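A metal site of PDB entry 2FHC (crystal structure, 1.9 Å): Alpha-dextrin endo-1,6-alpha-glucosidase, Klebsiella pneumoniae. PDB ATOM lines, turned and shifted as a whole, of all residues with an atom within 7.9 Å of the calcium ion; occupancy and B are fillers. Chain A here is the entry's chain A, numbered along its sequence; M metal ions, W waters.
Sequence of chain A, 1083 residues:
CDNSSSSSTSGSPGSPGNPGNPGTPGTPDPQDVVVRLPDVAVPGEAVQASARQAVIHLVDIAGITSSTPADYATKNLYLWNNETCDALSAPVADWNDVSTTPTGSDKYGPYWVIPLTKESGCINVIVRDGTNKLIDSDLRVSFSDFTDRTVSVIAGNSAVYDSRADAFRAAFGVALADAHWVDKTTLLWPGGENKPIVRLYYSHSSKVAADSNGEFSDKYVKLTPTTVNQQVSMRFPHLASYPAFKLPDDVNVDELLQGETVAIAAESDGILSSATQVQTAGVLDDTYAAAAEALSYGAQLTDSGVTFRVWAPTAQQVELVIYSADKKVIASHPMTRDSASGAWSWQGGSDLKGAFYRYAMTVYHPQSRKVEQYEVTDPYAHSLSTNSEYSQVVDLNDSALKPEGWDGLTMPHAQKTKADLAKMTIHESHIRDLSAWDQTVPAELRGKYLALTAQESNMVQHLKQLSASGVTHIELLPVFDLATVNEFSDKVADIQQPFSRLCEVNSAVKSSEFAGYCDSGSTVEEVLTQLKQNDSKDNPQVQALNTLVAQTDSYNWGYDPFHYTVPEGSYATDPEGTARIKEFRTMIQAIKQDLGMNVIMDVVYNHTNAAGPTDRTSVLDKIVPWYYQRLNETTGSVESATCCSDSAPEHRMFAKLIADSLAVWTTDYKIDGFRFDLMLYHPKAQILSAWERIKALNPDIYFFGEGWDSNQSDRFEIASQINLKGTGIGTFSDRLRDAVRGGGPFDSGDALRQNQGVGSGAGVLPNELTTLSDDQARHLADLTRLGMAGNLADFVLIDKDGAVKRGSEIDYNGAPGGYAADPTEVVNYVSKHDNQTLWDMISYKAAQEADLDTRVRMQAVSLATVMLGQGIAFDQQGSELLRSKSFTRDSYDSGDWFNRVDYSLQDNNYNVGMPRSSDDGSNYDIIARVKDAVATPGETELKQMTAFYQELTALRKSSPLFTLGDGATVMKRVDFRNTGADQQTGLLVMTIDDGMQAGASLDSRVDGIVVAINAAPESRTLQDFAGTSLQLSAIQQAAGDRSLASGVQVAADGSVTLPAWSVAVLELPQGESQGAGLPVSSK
Water W1 bridges the backbone carbonyl oxygen (O) of Val 485 (2.5 Å) and the side-chain carboxylate (OE1) of Glu 568 (2.7 Å).
OG of Ser 388 sits at hydrogen-bond distance from OD2 of Asp 481.
N of Phe 562 is in hydrogen-bond range of O of Asp 481, at 2.9 Å.
O of Asp 481 is in hydrogen-bond range of N of His 563 (3.3 Å).
N of Asp 481 lies within hydrogen-bond range of O of Val 566 (2.8 Å).
The backbone NH of Gly 569 sits close to the side-chain carboxylate of Glu 487 (2.9 Å).
The side-chain carboxylate (OE1) of Glu 487 lies within hydrogen-bond range of the backbone NH (N) of Asn 387.
NH2 of Arg 580 is in salt-bridge range of OE1 of Glu 487, 3.7 Å away.
The side-chain carboxylate (OE1) of Glu 568 sits at hydrogen-bond distance from the side-chain hydroxyl (OG) of Ser 570, 2.6 Å away.
Within 4 Å of the calcium ion: Asp 481, Leu 482, Glu 487 and Glu 568.
Along chain A the residues within 4 Å of the calcium ion span positions 481 to 568.
The nearest printed residue that does not touch the calcium ion is Ser 388 (4.1 Å).
The calcium ion is bound by OD1 of Asp 481 (2.3 Å), O of Leu 482 (2.4 Å), OE2 of Glu 487 (2.4 Å), water W1 (2.4 Å), water W2 (2.4 Å) and OE2 of Glu 568 (2.5 Å).
The calcium ion has six donor atoms within binding distance.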
ATOM      1  N   LEU A 384      -4.348   0.854  -9.648  1.00  0.00           N
ATOM      2  CA  LEU A 384      -3.922  -0.188 -10.582  1.00  0.00           C
ATOM      3  C   LEU A 384      -2.496  -0.028 -11.069  1.00  0.00           C
ATOM      4  O   LEU A 384      -1.895   1.038 -10.935  1.00  0.00           O
ATOM      5  CB  LEU A 384      -4.841  -0.178 -11.801  1.00  0.00           C
ATOM      6  CG  LEU A 384      -6.338  -0.468 -11.655  1.00  0.00           C
ATOM      7  CD1 LEU A 384      -7.101   0.104 -12.849  1.00  0.00           C
ATOM      8  CD2 LEU A 384      -6.563  -1.956 -11.531  1.00  0.00           C
ATOM      9  N   SER A 385      -1.955  -1.095 -11.646  1.00  0.00           N
ATOM     10  CA  SER A 385      -0.620  -1.056 -12.231  1.00  0.00           C
ATOM     11  C   SER A 385      -0.851  -0.616 -13.679  1.00  0.00           C
ATOM     12  O   SER A 385      -1.990  -0.397 -14.081  1.00  0.00           O
ATOM     13  CB  SER A 385       0.015  -2.458 -12.212  1.00  0.00           C
ATOM     14  OG  SER A 385      -0.654  -3.357 -13.085  1.00  0.00           O
ATOM     15  N   THR A 386       0.222  -0.492 -14.450  1.00  0.00           N
ATOM     16  CA  THR A 386       0.115  -0.076 -15.851  1.00  0.00           C
ATOM     17  C   THR A 386      -0.778  -1.005 -16.674  1.00  0.00           C
ATOM     18  O   THR A 386      -0.621  -2.224 -16.641  1.00  0.00           O
ATOM     19  CB  THR A 386       1.505  -0.001 -16.518  1.00  0.00           C
ATOM     20  OG1 THR A 386       2.340   0.908 -15.797  1.00  0.00           O
ATOM     21  CG2 THR A 386       1.370   0.480 -17.969  1.00  0.00           C
ATOM     22  N   ASN A 387      -1.700  -0.409 -17.416  1.00  0.00           N
ATOM     23  CA  ASN A 387      -2.653  -1.120 -18.273  1.00  0.00           C
ATOM     24  C   ASN A 387      -3.651  -1.991 -17.506  1.00  0.00           C
ATOM     25  O   ASN A 387      -4.253  -2.909 -18.066  1.00  0.00           O
ATOM     26  CB  ASN A 387      -1.915  -1.982 -19.316  1.00  0.00           C
ATOM     27  CG  ASN A 387      -2.620  -1.994 -20.669  1.00  0.00           C
ATOM     28  OD1 ASN A 387      -2.581  -3.000 -21.392  1.00  0.00           O
ATOM     29  ND2 ASN A 387      -3.264  -0.882 -21.026  1.00  0.00           N
ATOM     30  N   SER A 388      -3.821  -1.688 -16.218  1.00  0.00           N
ATOM     31  CA  SER A 388      -4.788  -2.392 -15.354  1.00  0.00           C
ATOM     32  C   SER A 388      -4.550  -3.884 -15.154  1.00  0.00           C
ATOM     33  O   SER A 388      -5.497  -4.622 -14.876  1.00  0.00           O
ATOM     34  CB  SER A 388      -6.210  -2.204 -15.905  1.00  0.00           C
ATOM     35  OG  SER A 388      -6.417  -0.887 -16.403  1.00  0.00           O
ATOM     36  N   PHE A 480     -12.485   7.544 -16.113  1.00  0.00           N
ATOM     37  CA  PHE A 480     -12.400   6.372 -15.246  1.00  0.00           C
ATOM     38  C   PHE A 480     -11.541   5.445 -16.102  1.00  0.00           C
ATOM     39  O   PHE A 480     -11.208   5.797 -17.229  1.00  0.00           O
ATOM     40  CB  PHE A 480     -13.784   5.771 -14.977  1.00  0.00           C
ATOM     41  CG  PHE A 480     -14.604   5.569 -16.220  1.00  0.00           C
ATOM     42  CD1 PHE A 480     -14.420   4.449 -17.024  1.00  0.00           C
ATOM     43  CD2 PHE A 480     -15.523   6.539 -16.620  1.00  0.00           C
ATOM     44  CE1 PHE A 480     -15.132   4.292 -18.200  1.00  0.00           C
ATOM     45  CE2 PHE A 480     -16.242   6.398 -17.812  1.00  0.00           C
ATOM     46  CZ  PHE A 480     -16.046   5.270 -18.596  1.00  0.00           C
ATOM     47  N   ASP A 481     -11.180   4.258 -15.595  1.00  0.00           N
ATOM     48  CA  ASP A 481     -10.315   3.355 -16.359  1.00  0.00           C
ATOM     49  C   ASP A 481     -10.953   2.724 -17.600  1.00  0.00           C
ATOM     50  O   ASP A 481     -11.750   1.783 -17.493  1.00  0.00           O
ATOM     51  CB  ASP A 481      -9.782   2.243 -15.434  1.00  0.00           C
ATOM     52  CG  ASP A 481      -8.828   1.301 -16.152  1.00  0.00           C
ATOM     53  OD1 ASP A 481      -8.014   1.767 -16.985  1.00  0.00           O
ATOM     54  OD2 ASP A 481      -8.855   0.080 -15.867  1.00  0.00           O
ATOM     55  N   LEU A 482     -10.595   3.235 -18.769  1.00  0.00           N
ATOM     56  CA  LEU A 482     -11.101   2.720 -20.043  1.00  0.00           C
ATOM     57  C   LEU A 482     -10.136   1.633 -20.535  1.00  0.00           C
ATOM     58  O   LEU A 482      -9.009   1.529 -20.059  1.00  0.00           O
ATOM     59  CB  LEU A 482     -11.226   3.855 -21.074  1.00  0.00           C
ATOM     60  CG  LEU A 482     -10.004   4.751 -21.332  1.00  0.00           C
ATOM     61  CD1 LEU A 482      -9.476   4.518 -22.743  1.00  0.00           C
ATOM     62  CD2 LEU A 482     -10.434   6.206 -21.167  1.00  0.00           C
ATOM     63  N   ALA A 483     -10.574   0.815 -21.485  1.00  0.00           N
ATOM     64  CA  ALA A 483      -9.724  -0.274 -21.948  1.00  0.00           C
ATOM     65  C   ALA A 483      -9.099  -0.097 -23.328  1.00  0.00           C
ATOM     66  O   ALA A 483      -8.074  -0.722 -23.627  1.00  0.00           O
ATOM     67  CB  ALA A 483     -10.524  -1.571 -21.935  1.00  0.00           C
ATOM     68  N   THR A 484      -9.680   0.772 -24.138  1.00  0.00           N
ATOM     69  CA  THR A 484      -9.246   0.950 -25.516  1.00  0.00           C
ATOM     70  C   THR A 484      -8.004   1.781 -25.875  1.00  0.00           C
ATOM     71  O   THR A 484      -7.830   2.175 -27.035  1.00  0.00           O
ATOM     72  CB  THR A 484     -10.444   1.407 -26.351  1.00  0.00           C
ATOM     73  OG1 THR A 484     -11.155   2.437 -25.664  1.00  0.00           O
ATOM     74  CG2 THR A 484     -11.397   0.225 -26.568  1.00  0.00           C
ATOM     75  N   VAL A 485      -7.149   2.026 -24.884  1.00  0.00           N
ATOM     76  CA  VAL A 485      -5.881   2.731 -25.089  1.00  0.00           C
ATOM     77  C   VAL A 485      -4.820   1.955 -24.293  1.00  0.00           C
ATOM     78  O   VAL A 485      -4.981   1.738 -23.095  1.00  0.00           O
ATOM     79  CB  VAL A 485      -5.908   4.186 -24.574  1.00  0.00           C
ATOM     80  CG1 VAL A 485      -4.480   4.761 -24.534  1.00  0.00           C
ATOM     81  CG2 VAL A 485      -6.779   5.057 -25.487  1.00  0.00           C
ATOM     82  N   ASN A 486      -3.752   1.521 -24.959  1.00  0.00           N
ATOM     83  CA  ASN A 486      -2.710   0.763 -24.260  1.00  0.00           C
ATOM     84  C   ASN A 486      -1.900   1.728 -23.393  1.00  0.00           C
ATOM     85  O   ASN A 486      -1.382   2.734 -23.882  1.00  0.00           O
ATOM     86  CB  ASN A 486      -1.791   0.067 -25.273  1.00  0.00           C
ATOM     87  CG  ASN A 486      -0.965  -1.048 -24.633  1.00  0.00           C
ATOM     88  OD1 ASN A 486      -0.326  -0.847 -23.600  1.00  0.00           O
ATOM     89  ND2 ASN A 486      -0.979  -2.218 -25.248  1.00  0.00           N
ATOM     90  N   GLU A 487      -1.801   1.423 -22.097  1.00  0.00           N
ATOM     91  CA  GLU A 487      -1.089   2.294 -21.185  1.00  0.00           C
ATOM     92  C   GLU A 487       0.434   2.082 -21.176  1.00  0.00           C
ATOM     93  O   GLU A 487       1.170   2.819 -20.528  1.00  0.00           O
ATOM     94  CB  GLU A 487      -1.683   2.182 -19.765  1.00  0.00           C
ATOM     95  CG  GLU A 487      -3.195   2.415 -19.752  1.00  0.00           C
ATOM     96  CD  GLU A 487      -3.793   2.545 -18.362  1.00  0.00           C
ATOM     97  OE1 GLU A 487      -3.167   2.096 -17.385  1.00  0.00           O
ATOM     98  OE2 GLU A 487      -4.919   3.095 -18.249  1.00  0.00           O
ATOM     99  N   ASP A 560     -15.600   2.590 -22.870  1.00  0.00           N
ATOM    100  CA  ASP A 560     -15.223   1.176 -22.787  1.00  0.00           C
ATOM    101  C   ASP A 560     -14.690   0.892 -21.372  1.00  0.00           C
ATOM    102  O   ASP A 560     -13.486   0.814 -21.169  1.00  0.00           O
ATOM    103  CB  ASP A 560     -14.134   0.910 -23.826  1.00  0.00           C
ATOM    104  CG  ASP A 560     -14.517   1.387 -25.217  1.00  0.00           C
ATOM    105  OD1 ASP A 560     -13.848   2.292 -25.770  1.00  0.00           O
ATOM    106  OD2 ASP A 560     -15.495   0.844 -25.772  1.00  0.00           O
ATOM    107  N   PHE A 562     -13.298  -0.583 -18.022  1.00  0.00           N
ATOM    108  CA  PHE A 562     -12.412  -1.664 -17.581  1.00  0.00           C
ATOM    109  C   PHE A 562     -12.579  -1.755 -16.059  1.00  0.00           C
ATOM    110  O   PHE A 562     -12.861  -2.827 -15.522  1.00  0.00           O
ATOM    111  CB  PHE A 562     -10.966  -1.344 -17.967  1.00  0.00           C
ATOM    112  CG  PHE A 562     -10.048  -2.541 -18.014  1.00  0.00           C
ATOM    113  CD1 PHE A 562      -8.810  -2.456 -18.650  1.00  0.00           C
ATOM    114  CD2 PHE A 562     -10.403  -3.742 -17.405  1.00  0.00           C
ATOM    115  CE1 PHE A 562      -7.944  -3.551 -18.688  1.00  0.00           C
ATOM    116  CE2 PHE A 562      -9.549  -4.838 -17.427  1.00  0.00           C
ATOM    117  CZ  PHE A 562      -8.311  -4.745 -18.074  1.00  0.00           C
ATOM    118  N   HIS A 563     -12.393  -0.628 -15.377  1.00  0.00           N
ATOM    119  CA  HIS A 563     -12.572  -0.533 -13.920  1.00  0.00           C
ATOM    120  C   HIS A 563     -13.343   0.762 -13.665  1.00  0.00           C
ATOM    121  O   HIS A 563     -12.945   1.837 -14.121  1.00  0.00           O
ATOM    122  CB  HIS A 563     -11.225  -0.507 -13.194  1.00  0.00           C
ATOM    123  CG  HIS A 563     -10.459  -1.788 -13.305  1.00  0.00           C
ATOM    124  ND1 HIS A 563     -10.658  -2.849 -12.455  1.00  0.00           N
ATOM    125  CD2 HIS A 563      -9.523  -2.184 -14.194  1.00  0.00           C
ATOM    126  CE1 HIS A 563      -9.883  -3.848 -12.814  1.00  0.00           C
ATOM    127  NE2 HIS A 563      -9.186  -3.478 -13.871  1.00  0.00           N
ATOM    128  N   VAL A 566     -11.403   3.773 -10.723  1.00  0.00           N
ATOM    129  CA  VAL A 566      -9.977   4.097 -10.769  1.00  0.00           C
ATOM    130  C   VAL A 566      -9.804   5.065 -11.938  1.00  0.00           C
ATOM    131  O   VAL A 566     -10.446   4.913 -12.980  1.00  0.00           O
ATOM    132  CB  VAL A 566      -9.094   2.859 -11.051  1.00  0.00           C
ATOM    133  CG1 VAL A 566      -7.607   3.248 -10.914  1.00  0.00           C
ATOM    134  CG2 VAL A 566      -9.432   1.722 -10.108  1.00  0.00           C
ATOM    135  N   PRO A 567      -8.976   6.107 -11.771  1.00  0.00           N
ATOM    136  CA  PRO A 567      -8.760   7.060 -12.852  1.00  0.00           C
ATOM    137  C   PRO A 567      -8.057   6.372 -14.025  1.00  0.00           C
ATOM    138  O   PRO A 567      -7.364   5.377 -13.832  1.00  0.00           O
ATOM    139  CB  PRO A 567      -7.865   8.119 -12.223  1.00  0.00           C
ATOM    140  CG  PRO A 567      -8.273   8.088 -10.777  1.00  0.00           C
ATOM    141  CD  PRO A 567      -8.394   6.613 -10.507  1.00  0.00           C
ATOM    142  N   GLU A 568      -8.238   6.895 -15.237  1.00  0.00           N
ATOM    143  CA  GLU A 568      -7.590   6.348 -16.435  1.00  0.00           C
ATOM    144  C   GLU A 568      -6.075   6.554 -16.284  1.00  0.00           C
ATOM    145  O   GLU A 568      -5.624   7.578 -15.782  1.00  0.00           O
ATOM    146  CB  GLU A 568      -8.103   7.072 -17.686  1.00  0.00           C
ATOM    147  CG  GLU A 568      -7.213   6.925 -18.926  1.00  0.00           C
ATOM    148  CD  GLU A 568      -7.072   5.489 -19.409  1.00  0.00           C
ATOM    149  OE1 GLU A 568      -6.243   5.250 -20.309  1.00  0.00           O
ATOM    150  OE2 GLU A 568      -7.776   4.597 -18.880  1.00  0.00           O
ATOM    151  N   GLY A 569      -5.289   5.574 -16.732  1.00  0.00           N
ATOM    152  CA  GLY A 569      -3.848   5.670 -16.605  1.00  0.00           C
ATOM    153  C   GLY A 569      -3.080   6.393 -17.691  1.00  0.00           C
ATOM    154  O   GLY A 569      -2.064   7.024 -17.419  1.00  0.00           O
ATOM    155  N   SER A 570      -3.560   6.311 -18.932  1.00  0.00           N
ATOM    156  CA  SER A 570      -2.876   6.968 -20.057  1.00  0.00           C
ATOM    157  C   SER A 570      -2.870   8.495 -19.951  1.00  0.00           C
ATOM    158  O   SER A 570      -2.054   9.144 -20.608  1.00  0.00           O
ATOM    159  CB  SER A 570      -3.509   6.540 -21.386  1.00  0.00           C
ATOM    160  OG  SER A 570      -4.794   7.093 -21.541  1.00  0.00           O
ATOM    161  N   TYR A 571      -3.771   9.053 -19.146  1.00  0.00           N
ATOM    162  CA  TYR A 571      -3.830  10.510 -18.981  1.00  0.00           C
ATOM    163  C   TYR A 571      -2.907  10.987 -17.861  1.00  0.00           C
ATOM    164  O   TYR A 571      -2.834  12.190 -17.580  1.00  0.00           O
ATOM    165  CB  TYR A 571      -5.279  10.961 -18.698  1.00  0.00           C
ATOM    166  CG  TYR A 571      -6.272  10.678 -19.824  1.00  0.00           C
ATOM    167  CD1 TYR A 571      -5.917  10.836 -21.161  1.00  0.00           C
ATOM    168  CD2 TYR A 571      -7.581  10.272 -19.534  1.00  0.00           C
ATOM    169  CE1 TYR A 571      -6.831  10.603 -22.192  1.00  0.00           C
ATOM    170  CE2 TYR A 571      -8.512  10.039 -20.564  1.00  0.00           C
ATOM    171  CZ  TYR A 571      -8.129  10.204 -21.881  1.00  0.00           C
ATOM    172  OH  TYR A 571      -9.032   9.972 -22.903  1.00  0.00           O
ATOM    173  N   ARG A 580      -1.264   8.328 -10.556  1.00  0.00           N
ATOM    174  CA  ARG A 580      -2.389   8.939 -11.278  1.00  0.00           C
ATOM    175  C   ARG A 580      -3.449   9.554 -10.370  1.00  0.00           C
ATOM    176  O   ARG A 580      -4.163  10.480 -10.767  1.00  0.00           O
ATOM    177  CB  ARG A 580      -3.057   7.915 -12.199  1.00  0.00           C
ATOM    178  CG  ARG A 580      -3.888   6.864 -11.455  1.00  0.00           C
ATOM    179  CD  ARG A 580      -4.493   5.831 -12.417  1.00  0.00           C
ATOM    180  NE  ARG A 580      -3.519   4.803 -12.812  1.00  0.00           N
ATOM    181  CZ  ARG A 580      -3.833   3.703 -13.495  1.00  0.00           C
ATOM    182  NH1 ARG A 580      -5.095   3.474 -13.851  1.00  0.00           N
ATOM    183  NH2 ARG A 580      -2.897   2.818 -13.806  1.00  0.00           N
ATOM    184  N   ARG A 616      -9.341 -10.364 -21.953  1.00  0.00           N
ATOM    185  CA  ARG A 616      -8.438  -9.680 -21.036  1.00  0.00           C
ATOM    186  C   ARG A 616      -9.158  -8.667 -20.149  1.00  0.00           C
ATOM    187  O   ARG A 616      -8.816  -8.512 -18.973  1.00  0.00           O
ATOM    188  CB  ARG A 616      -7.357  -8.943 -21.843  1.00  0.00           C
ATOM    189  CG  ARG A 616      -6.495  -7.979 -21.038  1.00  0.00           C
ATOM    190  CD  ARG A 616      -5.520  -7.224 -21.929  1.00  0.00           C
ATOM    191  NE  ARG A 616      -6.187  -6.284 -22.841  1.00  0.00           N
ATOM    192  CZ  ARG A 616      -6.334  -4.985 -22.605  1.00  0.00           C
ATOM    193  NH1 ARG A 616      -5.877  -4.452 -21.485  1.00  0.00           N
ATOM    194  NH2 ARG A 616      -6.956  -4.207 -23.488  1.00  0.00           N
HETATM  195 CA    CA M   1      -7.018   2.224 -19.010  1.00  0.00          CA
HETATM  196  O   HOH W   1      -6.429   2.762 -21.309  1.00  0.00           O
HETATM  197  O   HOH W   2      -6.076  -0.033 -19.101  1.00  0.00           O
